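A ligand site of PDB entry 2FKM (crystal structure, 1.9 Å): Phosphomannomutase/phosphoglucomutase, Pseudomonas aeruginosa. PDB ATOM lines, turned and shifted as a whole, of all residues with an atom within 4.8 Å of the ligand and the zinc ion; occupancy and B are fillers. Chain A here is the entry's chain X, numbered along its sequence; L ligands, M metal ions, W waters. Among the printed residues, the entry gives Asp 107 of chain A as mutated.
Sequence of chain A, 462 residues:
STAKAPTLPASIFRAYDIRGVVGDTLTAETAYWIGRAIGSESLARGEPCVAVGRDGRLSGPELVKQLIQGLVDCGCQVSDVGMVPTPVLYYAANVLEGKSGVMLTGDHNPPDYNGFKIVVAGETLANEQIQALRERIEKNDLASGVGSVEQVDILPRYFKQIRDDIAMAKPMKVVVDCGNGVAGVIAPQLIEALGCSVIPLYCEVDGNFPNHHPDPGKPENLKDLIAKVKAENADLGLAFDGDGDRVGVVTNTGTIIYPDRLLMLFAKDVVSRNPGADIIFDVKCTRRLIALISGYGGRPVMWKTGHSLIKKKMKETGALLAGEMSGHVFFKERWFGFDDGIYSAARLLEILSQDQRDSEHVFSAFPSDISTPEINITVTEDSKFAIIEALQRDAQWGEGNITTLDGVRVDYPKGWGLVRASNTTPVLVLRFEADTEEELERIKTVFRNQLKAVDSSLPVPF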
ATOM      1  N   ARG A  14      -1.766 -16.707  -5.780  1.00  0.00           N
ATOM      2  CA  ARG A  14      -2.035 -15.933  -6.983  1.00  0.00           C
ATOM      3  C   ARG A  14      -0.797 -15.197  -7.445  1.00  0.00           C
ATOM      4  O   ARG A  14       0.259 -15.254  -6.809  1.00  0.00           O
ATOM      5  CB  ARG A  14      -3.164 -14.933  -6.727  1.00  0.00           C
ATOM      6  CG  ARG A  14      -4.341 -15.515  -5.933  1.00  0.00           C
ATOM      7  CD  ARG A  14      -5.629 -14.781  -6.200  1.00  0.00           C
ATOM      8  NE  ARG A  14      -5.561 -13.362  -5.846  1.00  0.00           N
ATOM      9  CZ  ARG A  14      -6.508 -12.483  -6.171  1.00  0.00           C
ATOM     10  NH1 ARG A  14      -7.596 -12.878  -6.826  1.00  0.00           N
ATOM     11  NH2 ARG A  14      -6.382 -11.205  -5.827  1.00  0.00           N
ATOM     12  N   TYR A  16      -0.109 -11.928  -7.690  1.00  0.00           N
ATOM     13  CA  TYR A  16       0.293 -10.725  -6.946  1.00  0.00           C
ATOM     14  C   TYR A  16       0.287 -10.923  -5.448  1.00  0.00           C
ATOM     15  O   TYR A  16       0.874 -10.100  -4.725  1.00  0.00           O
ATOM     16  CB  TYR A  16      -0.621  -9.522  -7.223  1.00  0.00           C
ATOM     17  CG  TYR A  16      -0.996  -9.274  -8.682  1.00  0.00           C
ATOM     18  CD1 TYR A  16      -0.074  -9.403  -9.712  1.00  0.00           C
ATOM     19  CD2 TYR A  16      -2.273  -8.851  -9.015  1.00  0.00           C
ATOM     20  CE1 TYR A  16      -0.425  -9.160 -11.037  1.00  0.00           C
ATOM     21  CE2 TYR A  16      -2.638  -8.620 -10.351  1.00  0.00           C
ATOM     22  CZ  TYR A  16      -1.703  -8.761 -11.348  1.00  0.00           C
ATOM     23  OH  TYR A  16      -2.083  -8.536 -12.668  1.00  0.00           O
ATOM     24  N   ASP A  17      -0.383 -11.965  -4.978  1.00  0.00           N
ATOM     25  CA  ASP A  17      -0.635 -12.161  -3.551  1.00  0.00           C
ATOM     26  C   ASP A  17      -1.200 -13.554  -3.273  1.00  0.00           C
ATOM     27  O   ASP A  17      -1.168 -14.427  -4.141  1.00  0.00           O
ATOM     28  CB  ASP A  17      -1.625 -11.081  -3.066  1.00  0.00           C
ATOM     29  CG  ASP A  17      -3.016 -11.237  -3.661  1.00  0.00           C
ATOM     30  OD1 ASP A  17      -3.238 -12.194  -4.429  1.00  0.00           O
ATOM     31  OD2 ASP A  17      -3.890 -10.397  -3.378  1.00  0.00           O
ATOM     32  N   ARG A  19      -5.005 -15.044  -1.938  1.00  0.00           N
ATOM     33  CA  ARG A  19      -6.396 -14.633  -1.710  1.00  0.00           C
ATOM     34  C   ARG A  19      -7.287 -15.859  -1.705  1.00  0.00           C
ATOM     35  O   ARG A  19      -7.197 -16.690  -2.599  1.00  0.00           O
ATOM     36  CB  ARG A  19      -6.838 -13.654  -2.805  1.00  0.00           C
ATOM     37  CG  ARG A  19      -8.240 -13.036  -2.658  1.00  0.00           C
ATOM     38  CD  ARG A  19      -8.353 -11.945  -1.588  1.00  0.00           C
ATOM     39  NE  ARG A  19      -7.247 -10.984  -1.573  1.00  0.00           N
ATOM     40  CZ  ARG A  19      -7.183  -9.841  -2.265  1.00  0.00           C
ATOM     41  NH1 ARG A  19      -8.164  -9.441  -3.072  1.00  0.00           N
ATOM     42  NH2 ARG A  19      -6.115  -9.065  -2.139  1.00  0.00           N
ATOM     43  N   ASP A 107      -8.840  -6.992   0.852  1.00  0.00           N
ATOM     44  CA  ASP A 107      -8.919  -5.765   0.067  1.00  0.00           C
ATOM     45  C   ASP A 107     -10.384  -5.378  -0.170  1.00  0.00           C
ATOM     46  O   ASP A 107     -11.047  -5.017   0.805  1.00  0.00           O
ATOM     47  CB  ASP A 107      -8.089  -5.898  -1.213  1.00  0.00           C
ATOM     48  CG  ASP A 107      -7.730  -4.553  -1.804  1.00  0.00           C
ATOM     49  OD1 ASP A 107      -8.435  -3.562  -1.510  1.00  0.00           O
ATOM     50  OD2 ASP A 107      -6.729  -4.472  -2.562  1.00  0.00           O
ATOM     51  N   HIS A 108     -10.891  -5.456  -1.406  1.00  0.00           N
ATOM     52  CA  HIS A 108     -12.314  -5.125  -1.685  1.00  0.00           C
ATOM     53  C   HIS A 108     -13.152  -6.279  -2.223  1.00  0.00           C
ATOM     54  O   HIS A 108     -14.248  -6.063  -2.743  1.00  0.00           O
ATOM     55  CB  HIS A 108     -12.432  -3.919  -2.627  1.00  0.00           C
ATOM     56  CG  HIS A 108     -11.752  -4.098  -3.947  1.00  0.00           C
ATOM     57  ND1 HIS A 108     -10.501  -3.607  -4.207  1.00  0.00           N
ATOM     58  CD2 HIS A 108     -12.169  -4.696  -5.093  1.00  0.00           C
ATOM     59  CE1 HIS A 108     -10.153  -3.902  -5.441  1.00  0.00           C
ATOM     60  NE2 HIS A 108     -11.155  -4.566  -6.003  1.00  0.00           N
ATOM     61  N   LYS A 117      -0.753  -9.971   1.640  1.00  0.00           N
ATOM     62  CA  LYS A 117       0.190  -9.237   0.828  1.00  0.00           C
ATOM     63  C   LYS A 117       1.501  -9.234   1.568  1.00  0.00           C
ATOM     64  O   LYS A 117       1.548  -8.839   2.744  1.00  0.00           O
ATOM     65  CB  LYS A 117      -0.320  -7.823   0.556  1.00  0.00           C
ATOM     66  CG  LYS A 117      -1.526  -7.844  -0.414  1.00  0.00           C
ATOM     67  CD  LYS A 117      -2.007  -6.454  -0.766  1.00  0.00           C
ATOM     68  CE  LYS A 117      -3.407  -6.455  -1.333  1.00  0.00           C
ATOM     69  NZ  LYS A 117      -3.927  -5.073  -1.573  1.00  0.00           N
ATOM     70  N   ASP A 241     -10.084   2.386  -1.439  1.00  0.00           N
ATOM     71  CA  ASP A 241     -10.588   1.023  -1.558  1.00  0.00           C
ATOM     72  C   ASP A 241     -10.461   0.339  -0.207  1.00  0.00           C
ATOM     73  O   ASP A 241     -10.095   0.968   0.782  1.00  0.00           O
ATOM     74  CB  ASP A 241      -9.872   0.274  -2.679  1.00  0.00           C
ATOM     75  CG  ASP A 241      -8.508  -0.230  -2.285  1.00  0.00           C
ATOM     76  OD1 ASP A 241      -7.873   0.337  -1.393  1.00  0.00           O
ATOM     77  OD2 ASP A 241      -8.070  -1.207  -2.904  1.00  0.00           O
ATOM     78  N   ASP A 243      -8.460  -1.731   1.556  1.00  0.00           N
ATOM     79  CA  ASP A 243      -7.286  -1.682   2.436  1.00  0.00           C
ATOM     80  C   ASP A 243      -6.460  -0.393   2.309  1.00  0.00           C
ATOM     81  O   ASP A 243      -5.453  -0.243   3.003  1.00  0.00           O
ATOM     82  CB  ASP A 243      -6.424  -2.937   2.263  1.00  0.00           C
ATOM     83  CG  ASP A 243      -5.661  -2.985   0.943  1.00  0.00           C
ATOM     84  OD1 ASP A 243      -5.665  -1.994   0.183  1.00  0.00           O
ATOM     85  OD2 ASP A 243      -5.051  -4.034   0.686  1.00  0.00           O
ATOM     86  N   ASP A 245      -4.774   0.998  -0.385  1.00  0.00           N
ATOM     87  CA  ASP A 245      -3.701   1.104  -1.405  1.00  0.00           C
ATOM     88  C   ASP A 245      -4.132   1.607  -2.784  1.00  0.00           C
ATOM     89  O   ASP A 245      -3.273   1.787  -3.652  1.00  0.00           O
ATOM     90  CB  ASP A 245      -2.886  -0.191  -1.508  1.00  0.00           C
ATOM     91  CG  ASP A 245      -3.683  -1.368  -2.009  1.00  0.00           C
ATOM     92  OD1 ASP A 245      -4.801  -1.169  -2.517  1.00  0.00           O
ATOM     93  OD2 ASP A 245      -3.193  -2.495  -1.900  1.00  0.00           O
ATOM     94  N   ARG A 246      -5.427   1.831  -2.979  1.00  0.00           N
ATOM     95  CA  ARG A 246      -5.971   2.500  -4.156  1.00  0.00           C
ATOM     96  C   ARG A 246      -6.681   3.787  -3.740  1.00  0.00           C
ATOM     97  O   ARG A 246      -7.323   3.856  -2.689  1.00  0.00           O
ATOM     98  CB  ARG A 246      -7.004   1.637  -4.912  1.00  0.00           C
ATOM     99  CG  ARG A 246      -6.500   0.333  -5.532  1.00  0.00           C
ATOM    100  CD  ARG A 246      -7.598  -0.281  -6.411  1.00  0.00           C
ATOM    101  NE  ARG A 246      -7.331  -1.671  -6.790  1.00  0.00           N
ATOM    102  CZ  ARG A 246      -7.946  -2.326  -7.768  1.00  0.00           C
ATOM    103  NH1 ARG A 246      -8.894  -1.743  -8.508  1.00  0.00           N
ATOM    104  NH2 ARG A 246      -7.628  -3.587  -8.013  1.00  0.00           N
ATOM    105  N   LYS A 284      -2.222  -0.223 -19.138  1.00  0.00           N
ATOM    106  CA  LYS A 284      -3.579   0.301 -19.243  1.00  0.00           C
ATOM    107  C   LYS A 284      -3.682   1.819 -19.229  1.00  0.00           C
ATOM    108  O   LYS A 284      -4.776   2.347 -19.383  1.00  0.00           O
ATOM    109  CB  LYS A 284      -4.445  -0.228 -18.099  1.00  0.00           C
ATOM    110  CG  LYS A 284      -4.742  -1.716 -18.223  1.00  0.00           C
ATOM    111  CD  LYS A 284      -5.121  -2.327 -16.885  1.00  0.00           C
ATOM    112  CE  LYS A 284      -6.408  -1.748 -16.343  1.00  0.00           C
ATOM    113  NZ  LYS A 284      -6.621  -2.221 -14.932  1.00  0.00           N
ATOM    114  N   THR A 305       0.804  -4.629 -15.538  1.00  0.00           N
ATOM    115  CA  THR A 305      -0.198  -4.397 -14.525  1.00  0.00           C
ATOM    116  C   THR A 305       0.066  -5.311 -13.341  1.00  0.00           C
ATOM    117  O   THR A 305       0.522  -6.446 -13.524  1.00  0.00           O
ATOM    118  CB  THR A 305      -1.575  -4.699 -15.086  1.00  0.00           C
ATOM    119  OG1 THR A 305      -1.836  -3.809 -16.168  1.00  0.00           O
ATOM    120  CG2 THR A 305      -2.649  -4.600 -13.999  1.00  0.00           C
ATOM    121  N   GLY A 306      -0.245  -4.841 -12.141  1.00  0.00           N
ATOM    122  CA  GLY A 306      -0.076  -5.622 -10.908  1.00  0.00           C
ATOM    123  C   GLY A 306       0.880  -4.942  -9.932  1.00  0.00           C
ATOM    124  O   GLY A 306       2.043  -4.734 -10.252  1.00  0.00           O
ATOM    125  N   HIS A 307       0.385  -4.618  -8.731  1.00  0.00           N
ATOM    126  CA  HIS A 307       1.144  -3.771  -7.784  1.00  0.00           C
ATOM    127  C   HIS A 307       2.497  -4.353  -7.375  1.00  0.00           C
ATOM    128  O   HIS A 307       3.463  -3.600  -7.200  1.00  0.00           O
ATOM    129  CB  HIS A 307       0.308  -3.447  -6.529  1.00  0.00           C
ATOM    130  CG  HIS A 307      -0.003  -4.641  -5.693  1.00  0.00           C
ATOM    131  ND1 HIS A 307       0.725  -4.969  -4.566  1.00  0.00           N
ATOM    132  CD2 HIS A 307      -0.943  -5.600  -5.817  1.00  0.00           C
ATOM    133  CE1 HIS A 307       0.242  -6.076  -4.037  1.00  0.00           C
ATOM    134  NE2 HIS A 307      -0.773  -6.477  -4.777  1.00  0.00           N
ATOM    135  N   GLU A 324      -0.671   2.727 -11.513  1.00  0.00           N
ATOM    136  CA  GLU A 324      -1.477   1.839 -12.316  1.00  0.00           C
ATOM    137  C   GLU A 324      -2.818   2.504 -12.542  1.00  0.00           C
ATOM    138  O   GLU A 324      -3.263   3.286 -11.699  1.00  0.00           O
ATOM    139  CB  GLU A 324      -1.789   0.543 -11.584  1.00  0.00           C
ATOM    140  CG  GLU A 324      -0.636  -0.302 -11.214  1.00  0.00           C
ATOM    141  CD  GLU A 324      -1.092  -1.658 -10.754  1.00  0.00           C
ATOM    142  OE1 GLU A 324      -1.314  -2.498 -11.621  1.00  0.00           O
ATOM    143  OE2 GLU A 324      -1.260  -1.856  -9.538  1.00  0.00           O
ATOM    144  N   SER A 326      -5.663   1.142 -12.206  1.00  0.00           N
ATOM    145  CA  SER A 326      -6.607   0.719 -11.181  1.00  0.00           C
ATOM    146  C   SER A 326      -6.544   1.571  -9.931  1.00  0.00           C
ATOM    147  O   SER A 326      -7.400   1.452  -9.065  1.00  0.00           O
ATOM    148  CB  SER A 326      -6.342  -0.732 -10.785  1.00  0.00           C
ATOM    149  OG  SER A 326      -5.006  -0.853 -10.369  1.00  0.00           O
ATOM    150  N   HIS A 328      -3.536   2.252  -7.878  1.00  0.00           N
ATOM    151  CA  HIS A 328      -2.338   2.148  -7.057  1.00  0.00           C
ATOM    152  C   HIS A 328      -1.307   3.139  -7.573  1.00  0.00           C
ATOM    153  O   HIS A 328      -0.925   3.061  -8.736  1.00  0.00           O
ATOM    154  CB  HIS A 328      -1.738   0.757  -7.165  1.00  0.00           C
ATOM    155  CG  HIS A 328      -2.590  -0.347  -6.614  1.00  0.00           C
ATOM    156  ND1 HIS A 328      -3.640  -0.892  -7.314  1.00  0.00           N
ATOM    157  CD2 HIS A 328      -2.507  -1.042  -5.458  1.00  0.00           C
ATOM    158  CE1 HIS A 328      -4.186  -1.859  -6.598  1.00  0.00           C
ATOM    159  NE2 HIS A 328      -3.507  -1.977  -5.472  1.00  0.00           N
ATOM    160  N   ARG A 420      -4.966  -7.601 -22.666  1.00  0.00           N
ATOM    161  CA  ARG A 420      -4.116  -8.424 -21.830  1.00  0.00           C
ATOM    162  C   ARG A 420      -4.969  -9.396 -21.036  1.00  0.00           C
ATOM    163  O   ARG A 420      -6.183  -9.238 -20.939  1.00  0.00           O
ATOM    164  CB  ARG A 420      -3.314  -7.545 -20.876  1.00  0.00           C
ATOM    165  CG  ARG A 420      -4.189  -6.691 -19.994  1.00  0.00           C
ATOM    166  CD  ARG A 420      -3.359  -5.955 -18.992  1.00  0.00           C
ATOM    167  NE  ARG A 420      -2.814  -6.858 -17.975  1.00  0.00           N
ATOM    168  CZ  ARG A 420      -3.432  -7.219 -16.860  1.00  0.00           C
ATOM    169  NH1 ARG A 420      -4.663  -6.819 -16.575  1.00  0.00           N
ATOM    170  NH2 ARG A 420      -2.807  -8.019 -16.019  1.00  0.00           N
ATOM    171  N   ALA A 421      -4.316 -10.411 -20.472  1.00  0.00           N
ATOM    172  CA  ALA A 421      -4.959 -11.361 -19.564  1.00  0.00           C
ATOM    173  C   ALA A 421      -4.894 -10.868 -18.115  1.00  0.00           C
ATOM    174  O   ALA A 421      -3.830 -10.476 -17.621  1.00  0.00           O
ATOM    175  CB  ALA A 421      -4.295 -12.720 -19.658  1.00  0.00           C
ATOM    176  N   SER A 422      -6.032 -10.888 -17.421  1.00  0.00           N
ATOM    177  CA  SER A 422      -6.081 -10.605 -15.995  1.00  0.00           C
ATOM    178  C   SER A 422      -5.316 -11.676 -15.244  1.00  0.00           C
ATOM    179  O   SER A 422      -5.344 -12.848 -15.638  1.00  0.00           O
ATOM    180  CB  SER A 422      -7.538 -10.594 -15.507  1.00  0.00           C
ATOM    181  OG  SER A 422      -7.638 -10.540 -14.090  1.00  0.00           O
ATOM    182  N   ASN A 423      -4.636 -11.297 -14.164  1.00  0.00           N
ATOM    183  CA  ASN A 423      -4.013 -12.281 -13.278  1.00  0.00           C
ATOM    184  C   ASN A 423      -4.837 -12.565 -12.033  1.00  0.00           C
ATOM    185  O   ASN A 423      -4.387 -13.288 -11.136  1.00  0.00           O
ATOM    186  CB  ASN A 423      -2.604 -11.830 -12.884  1.00  0.00           C
ATOM    187  CG  ASN A 423      -1.632 -11.853 -14.046  1.00  0.00           C
ATOM    188  OD1 ASN A 423      -1.367 -12.893 -14.620  1.00  0.00           O
ATOM    189  ND2 ASN A 423      -1.088 -10.696 -14.389  1.00  0.00           N
ATOM    190  N   THR A 424      -6.027 -11.984 -11.946  1.00  0.00           N
ATOM    191  CA  THR A 424      -6.902 -12.198 -10.796  1.00  0.00           C
ATOM    192  C   THR A 424      -8.262 -12.819 -11.155  1.00  0.00           C
ATOM    193  O   THR A 424      -8.950 -13.338 -10.275  1.00  0.00           O
ATOM    194  CB  THR A 424      -7.120 -10.900 -10.000  1.00  0.00           C
ATOM    195  OG1 THR A 424      -7.687  -9.887 -10.850  1.00  0.00           O
ATOM    196  CG2 THR A 424      -5.806 -10.385  -9.398  1.00  0.00           C
ATOM    197  N   THR A 425      -8.643 -12.788 -12.428  1.00  0.00           N
ATOM    198  CA  THR A 425      -9.899 -13.363 -12.901  1.00  0.00           C
ATOM    199  C   THR A 425      -9.710 -13.995 -14.285  1.00  0.00           C
ATOM    200  O   THR A 425      -8.784 -13.640 -15.004  1.00  0.00           O
ATOM    201  CB  THR A 425     -11.009 -12.289 -12.968  1.00  0.00           C
ATOM    202  OG1 THR A 425     -10.569 -11.212 -13.791  1.00  0.00           O
ATOM    203  CG2 THR A 425     -11.352 -11.763 -11.579  1.00  0.00           C
ATOM    204  N   VAL A 429      -8.724  -8.243 -20.535  1.00  0.00           N
ATOM    205  CA  VAL A 429      -8.897  -6.838 -20.196  1.00  0.00           C
ATOM    206  C   VAL A 429      -8.463  -5.980 -21.390  1.00  0.00           C
ATOM    207  O   VAL A 429      -7.351  -6.150 -21.912  1.00  0.00           O
ATOM    208  CB  VAL A 429      -8.036  -6.417 -18.979  1.00  0.00           C
ATOM    209  CG1 VAL A 429      -8.153  -4.912 -18.719  1.00  0.00           C
ATOM    210  CG2 VAL A 429      -8.448  -7.201 -17.740  1.00  0.00           C
HETATM  211  C1  LIG L   1      -4.377  -5.616  -8.419  1.00  0.00           C
HETATM  212  C2  LIG L   1      -3.546  -4.793  -9.413  1.00  0.00           C
HETATM  213  C3  LIG L   1      -4.414  -3.877 -10.254  1.00  0.00           C
HETATM  214  C4  LIG L   1      -5.240  -4.772 -11.123  1.00  0.00           C
HETATM  215  C5  LIG L   1      -6.080  -5.699 -10.239  1.00  0.00           C
HETATM  216  C6  LIG L   1      -5.952  -7.109 -10.747  1.00  0.00           C
HETATM  217  O1  LIG L   1      -4.353  -5.000  -7.131  1.00  0.00           O
HETATM  218  O2  LIG L   1      -2.571  -4.022  -8.735  1.00  0.00           O
HETATM  219  O3  LIG L   1      -3.684  -3.039 -11.136  1.00  0.00           O
HETATM  220  O4  LIG L   1      -6.050  -4.033 -12.023  1.00  0.00           O
HETATM  221  O5  LIG L   1      -5.736  -5.715  -8.847  1.00  0.00           O
HETATM  222  O6  LIG L   1      -5.167  -7.055 -11.926  1.00  0.00           O
HETATM  223  P1  LIG L   1      -5.587  -7.779 -13.153  1.00  0.00           P
HETATM  224  O7  LIG L   1      -4.426  -8.621 -13.578  1.00  0.00           O
HETATM  225  O8  LIG L   1      -5.951  -6.790 -14.199  1.00  0.00           O
HETATM  226  O9  LIG L   1      -6.756  -8.661 -12.825  1.00  0.00           O
HETATM  227  P2  LIG L   1      -4.726  -5.660  -5.816  1.00  0.00           P
HETATM  228  O10 LIG L   1      -6.147  -5.349  -5.435  1.00  0.00           O
HETATM  229  O11 LIG L   1      -3.841  -5.094  -4.743  1.00  0.00           O
HETATM  230  O12 LIG L   1      -4.550  -7.160  -5.864  1.00  0.00           O
HETATM  231 ZN    ZN M   1      -6.413  -2.341  -2.481  1.00  0.00          ZN
HETATM  232  O   HOH W   1      -4.058  -1.344 -13.398  1.00  0.00           O
HETATM  233  O   HOH W   2      -8.892  -7.224 -13.688  1.00  0.00           O
HETATM  234  O   HOH W   3      -7.770  -7.095  -6.868  1.00  0.00           O
HETATM  235  O   HOH W   4      -7.313  -5.031 -15.193  1.00  0.00           O
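Water W4 lies within hydrogen-bond range of O8 of the ligand (2.4 Å), NZ of Lys 284 (2.9 Å) and NH1 of Arg 420 (3.5 Å). Water W1 lies within hydrogen-bond range of an oxygen (O3) of the ligand, the side-chain amino group (NZ) of Lys 284, the backbone NH (N) of Ser 326 and the side-chain carboxylate (OE1) of Glu 324.
An oxygen (O10) of the ligand sits close to the side-chain carboxylate of Asp 107 (3.1 Å). An oxygen (O9) of the ligand lies within hydrogen-bond range of the side-chain hydroxyl (OG) of Ser 422. The side-chain carboxylate (OE1) of Glu 324 is in hydrogen-bond range of an oxygen (O3) of the ligand (2.5 Å). OG1 of Thr 424 sits at hydrogen-bond distance from O9 of the ligand (2.5 Å). OH of Tyr 16 is in hydrogen-bond range of O7 of the ligand (2.5 Å). An oxygen (O3) of the ligand sits at hydrogen-bond distance from the side-chain hydroxyl of Ser 326. O8 of the ligand lies within salt-bridge range of NH1 of Arg 420 (2.7 Å). The backbone NH (N) of Asn 423 is in hydrogen-bond range of an oxygen (O7) of the ligand (2.7 Å). The guanidinium group (NH2) of Arg 246 is in salt-bridge range of an oxygen (O10) of the ligand (3.5 Å). N of His 307 sits at hydrogen-bond distance from O2 of the ligand, 3.0 Å away. A ring nitrogen (NE2) of His 307 lies close to an oxygen (O11) of the ligand. An oxygen (O11) of the ligand lies within salt-bridge range of the side-chain amino group (NZ) of Lys 117. NE2 of His 328 is in hydrogen-bond range of O11 of the ligand (3.2 Å). An oxygen (O4) of the ligand lies within hydrogen-bond range of the side-chain amino group (NZ) of Lys 284, 3.5 Å away.
Thr 305 touches the ligand. Gly 306 touches the ligand (CA to O2, 3.7 Å). 16 residues have an atom within 4 Å of the ligand: Tyr 16, Asp 107, Lys 117, Asp 245, Arg 246, Lys 284, Thr 305, Gly 306, His 307, Glu 324, Ser 326, His 328, Arg 420, Ser 422, Asn 423 and Thr 424. The nearest printed residue that does not touch the ligand is Asp 17 (4.1 Å).
The zinc ion is bound by the side-chain carboxylate (OD1) of Asp 245 (2.0 Å), the side-chain carboxylate (OD2) of Asp 241 (2.1 Å), the side-chain carboxylate (OD2) of Asp 107 (2.2 Å) and the side-chain carboxylate (OD1) of Asp 107 (2.6 Å). Slightly farther from the zinc ion lies the side-chain carboxylate (OD1) of Asp 243 (2.8 Å).
Lys 117 touches the zinc ion (NZ to ZN, 3.8 Å). The nearest printed residue that does not touch the zinc ion is Arg 246 (4.1 Å).
The backbone NH of Asp 245 sits close to the side-chain carboxylate of Asp 243. The side-chain carboxylate (OD1) of Asp 241 is in hydrogen-bond range of the backbone NH (N) of Arg 246, at 3.3 Å. OD1 of Asp 107 sits close to ND1 of His 108 (3.4 Å). The side-chain carboxylate (OE2) of Glu 324 sits at hydrogen-bond distance from the backbone NH (N) of His 307 (3.3 Å). The side-chain carboxylate (OE2) of Glu 324 is in hydrogen-bond range of a ring nitrogen (ND1) of His 328 (3.4 Å). The backbone NH (N) of Gly 306 lies within hydrogen-bond range of the side-chain carboxylate (OE1) of Glu 324, at 2.6 Å. NH2 of Arg 420 lies within hydrogen-bond range of OH of Tyr 16 (3.5 Å). The backbone carbonyl oxygen (O) of Arg 420 lies within hydrogen-bond range of the backbone NH (N) of Val 429, at 2.8 Å.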
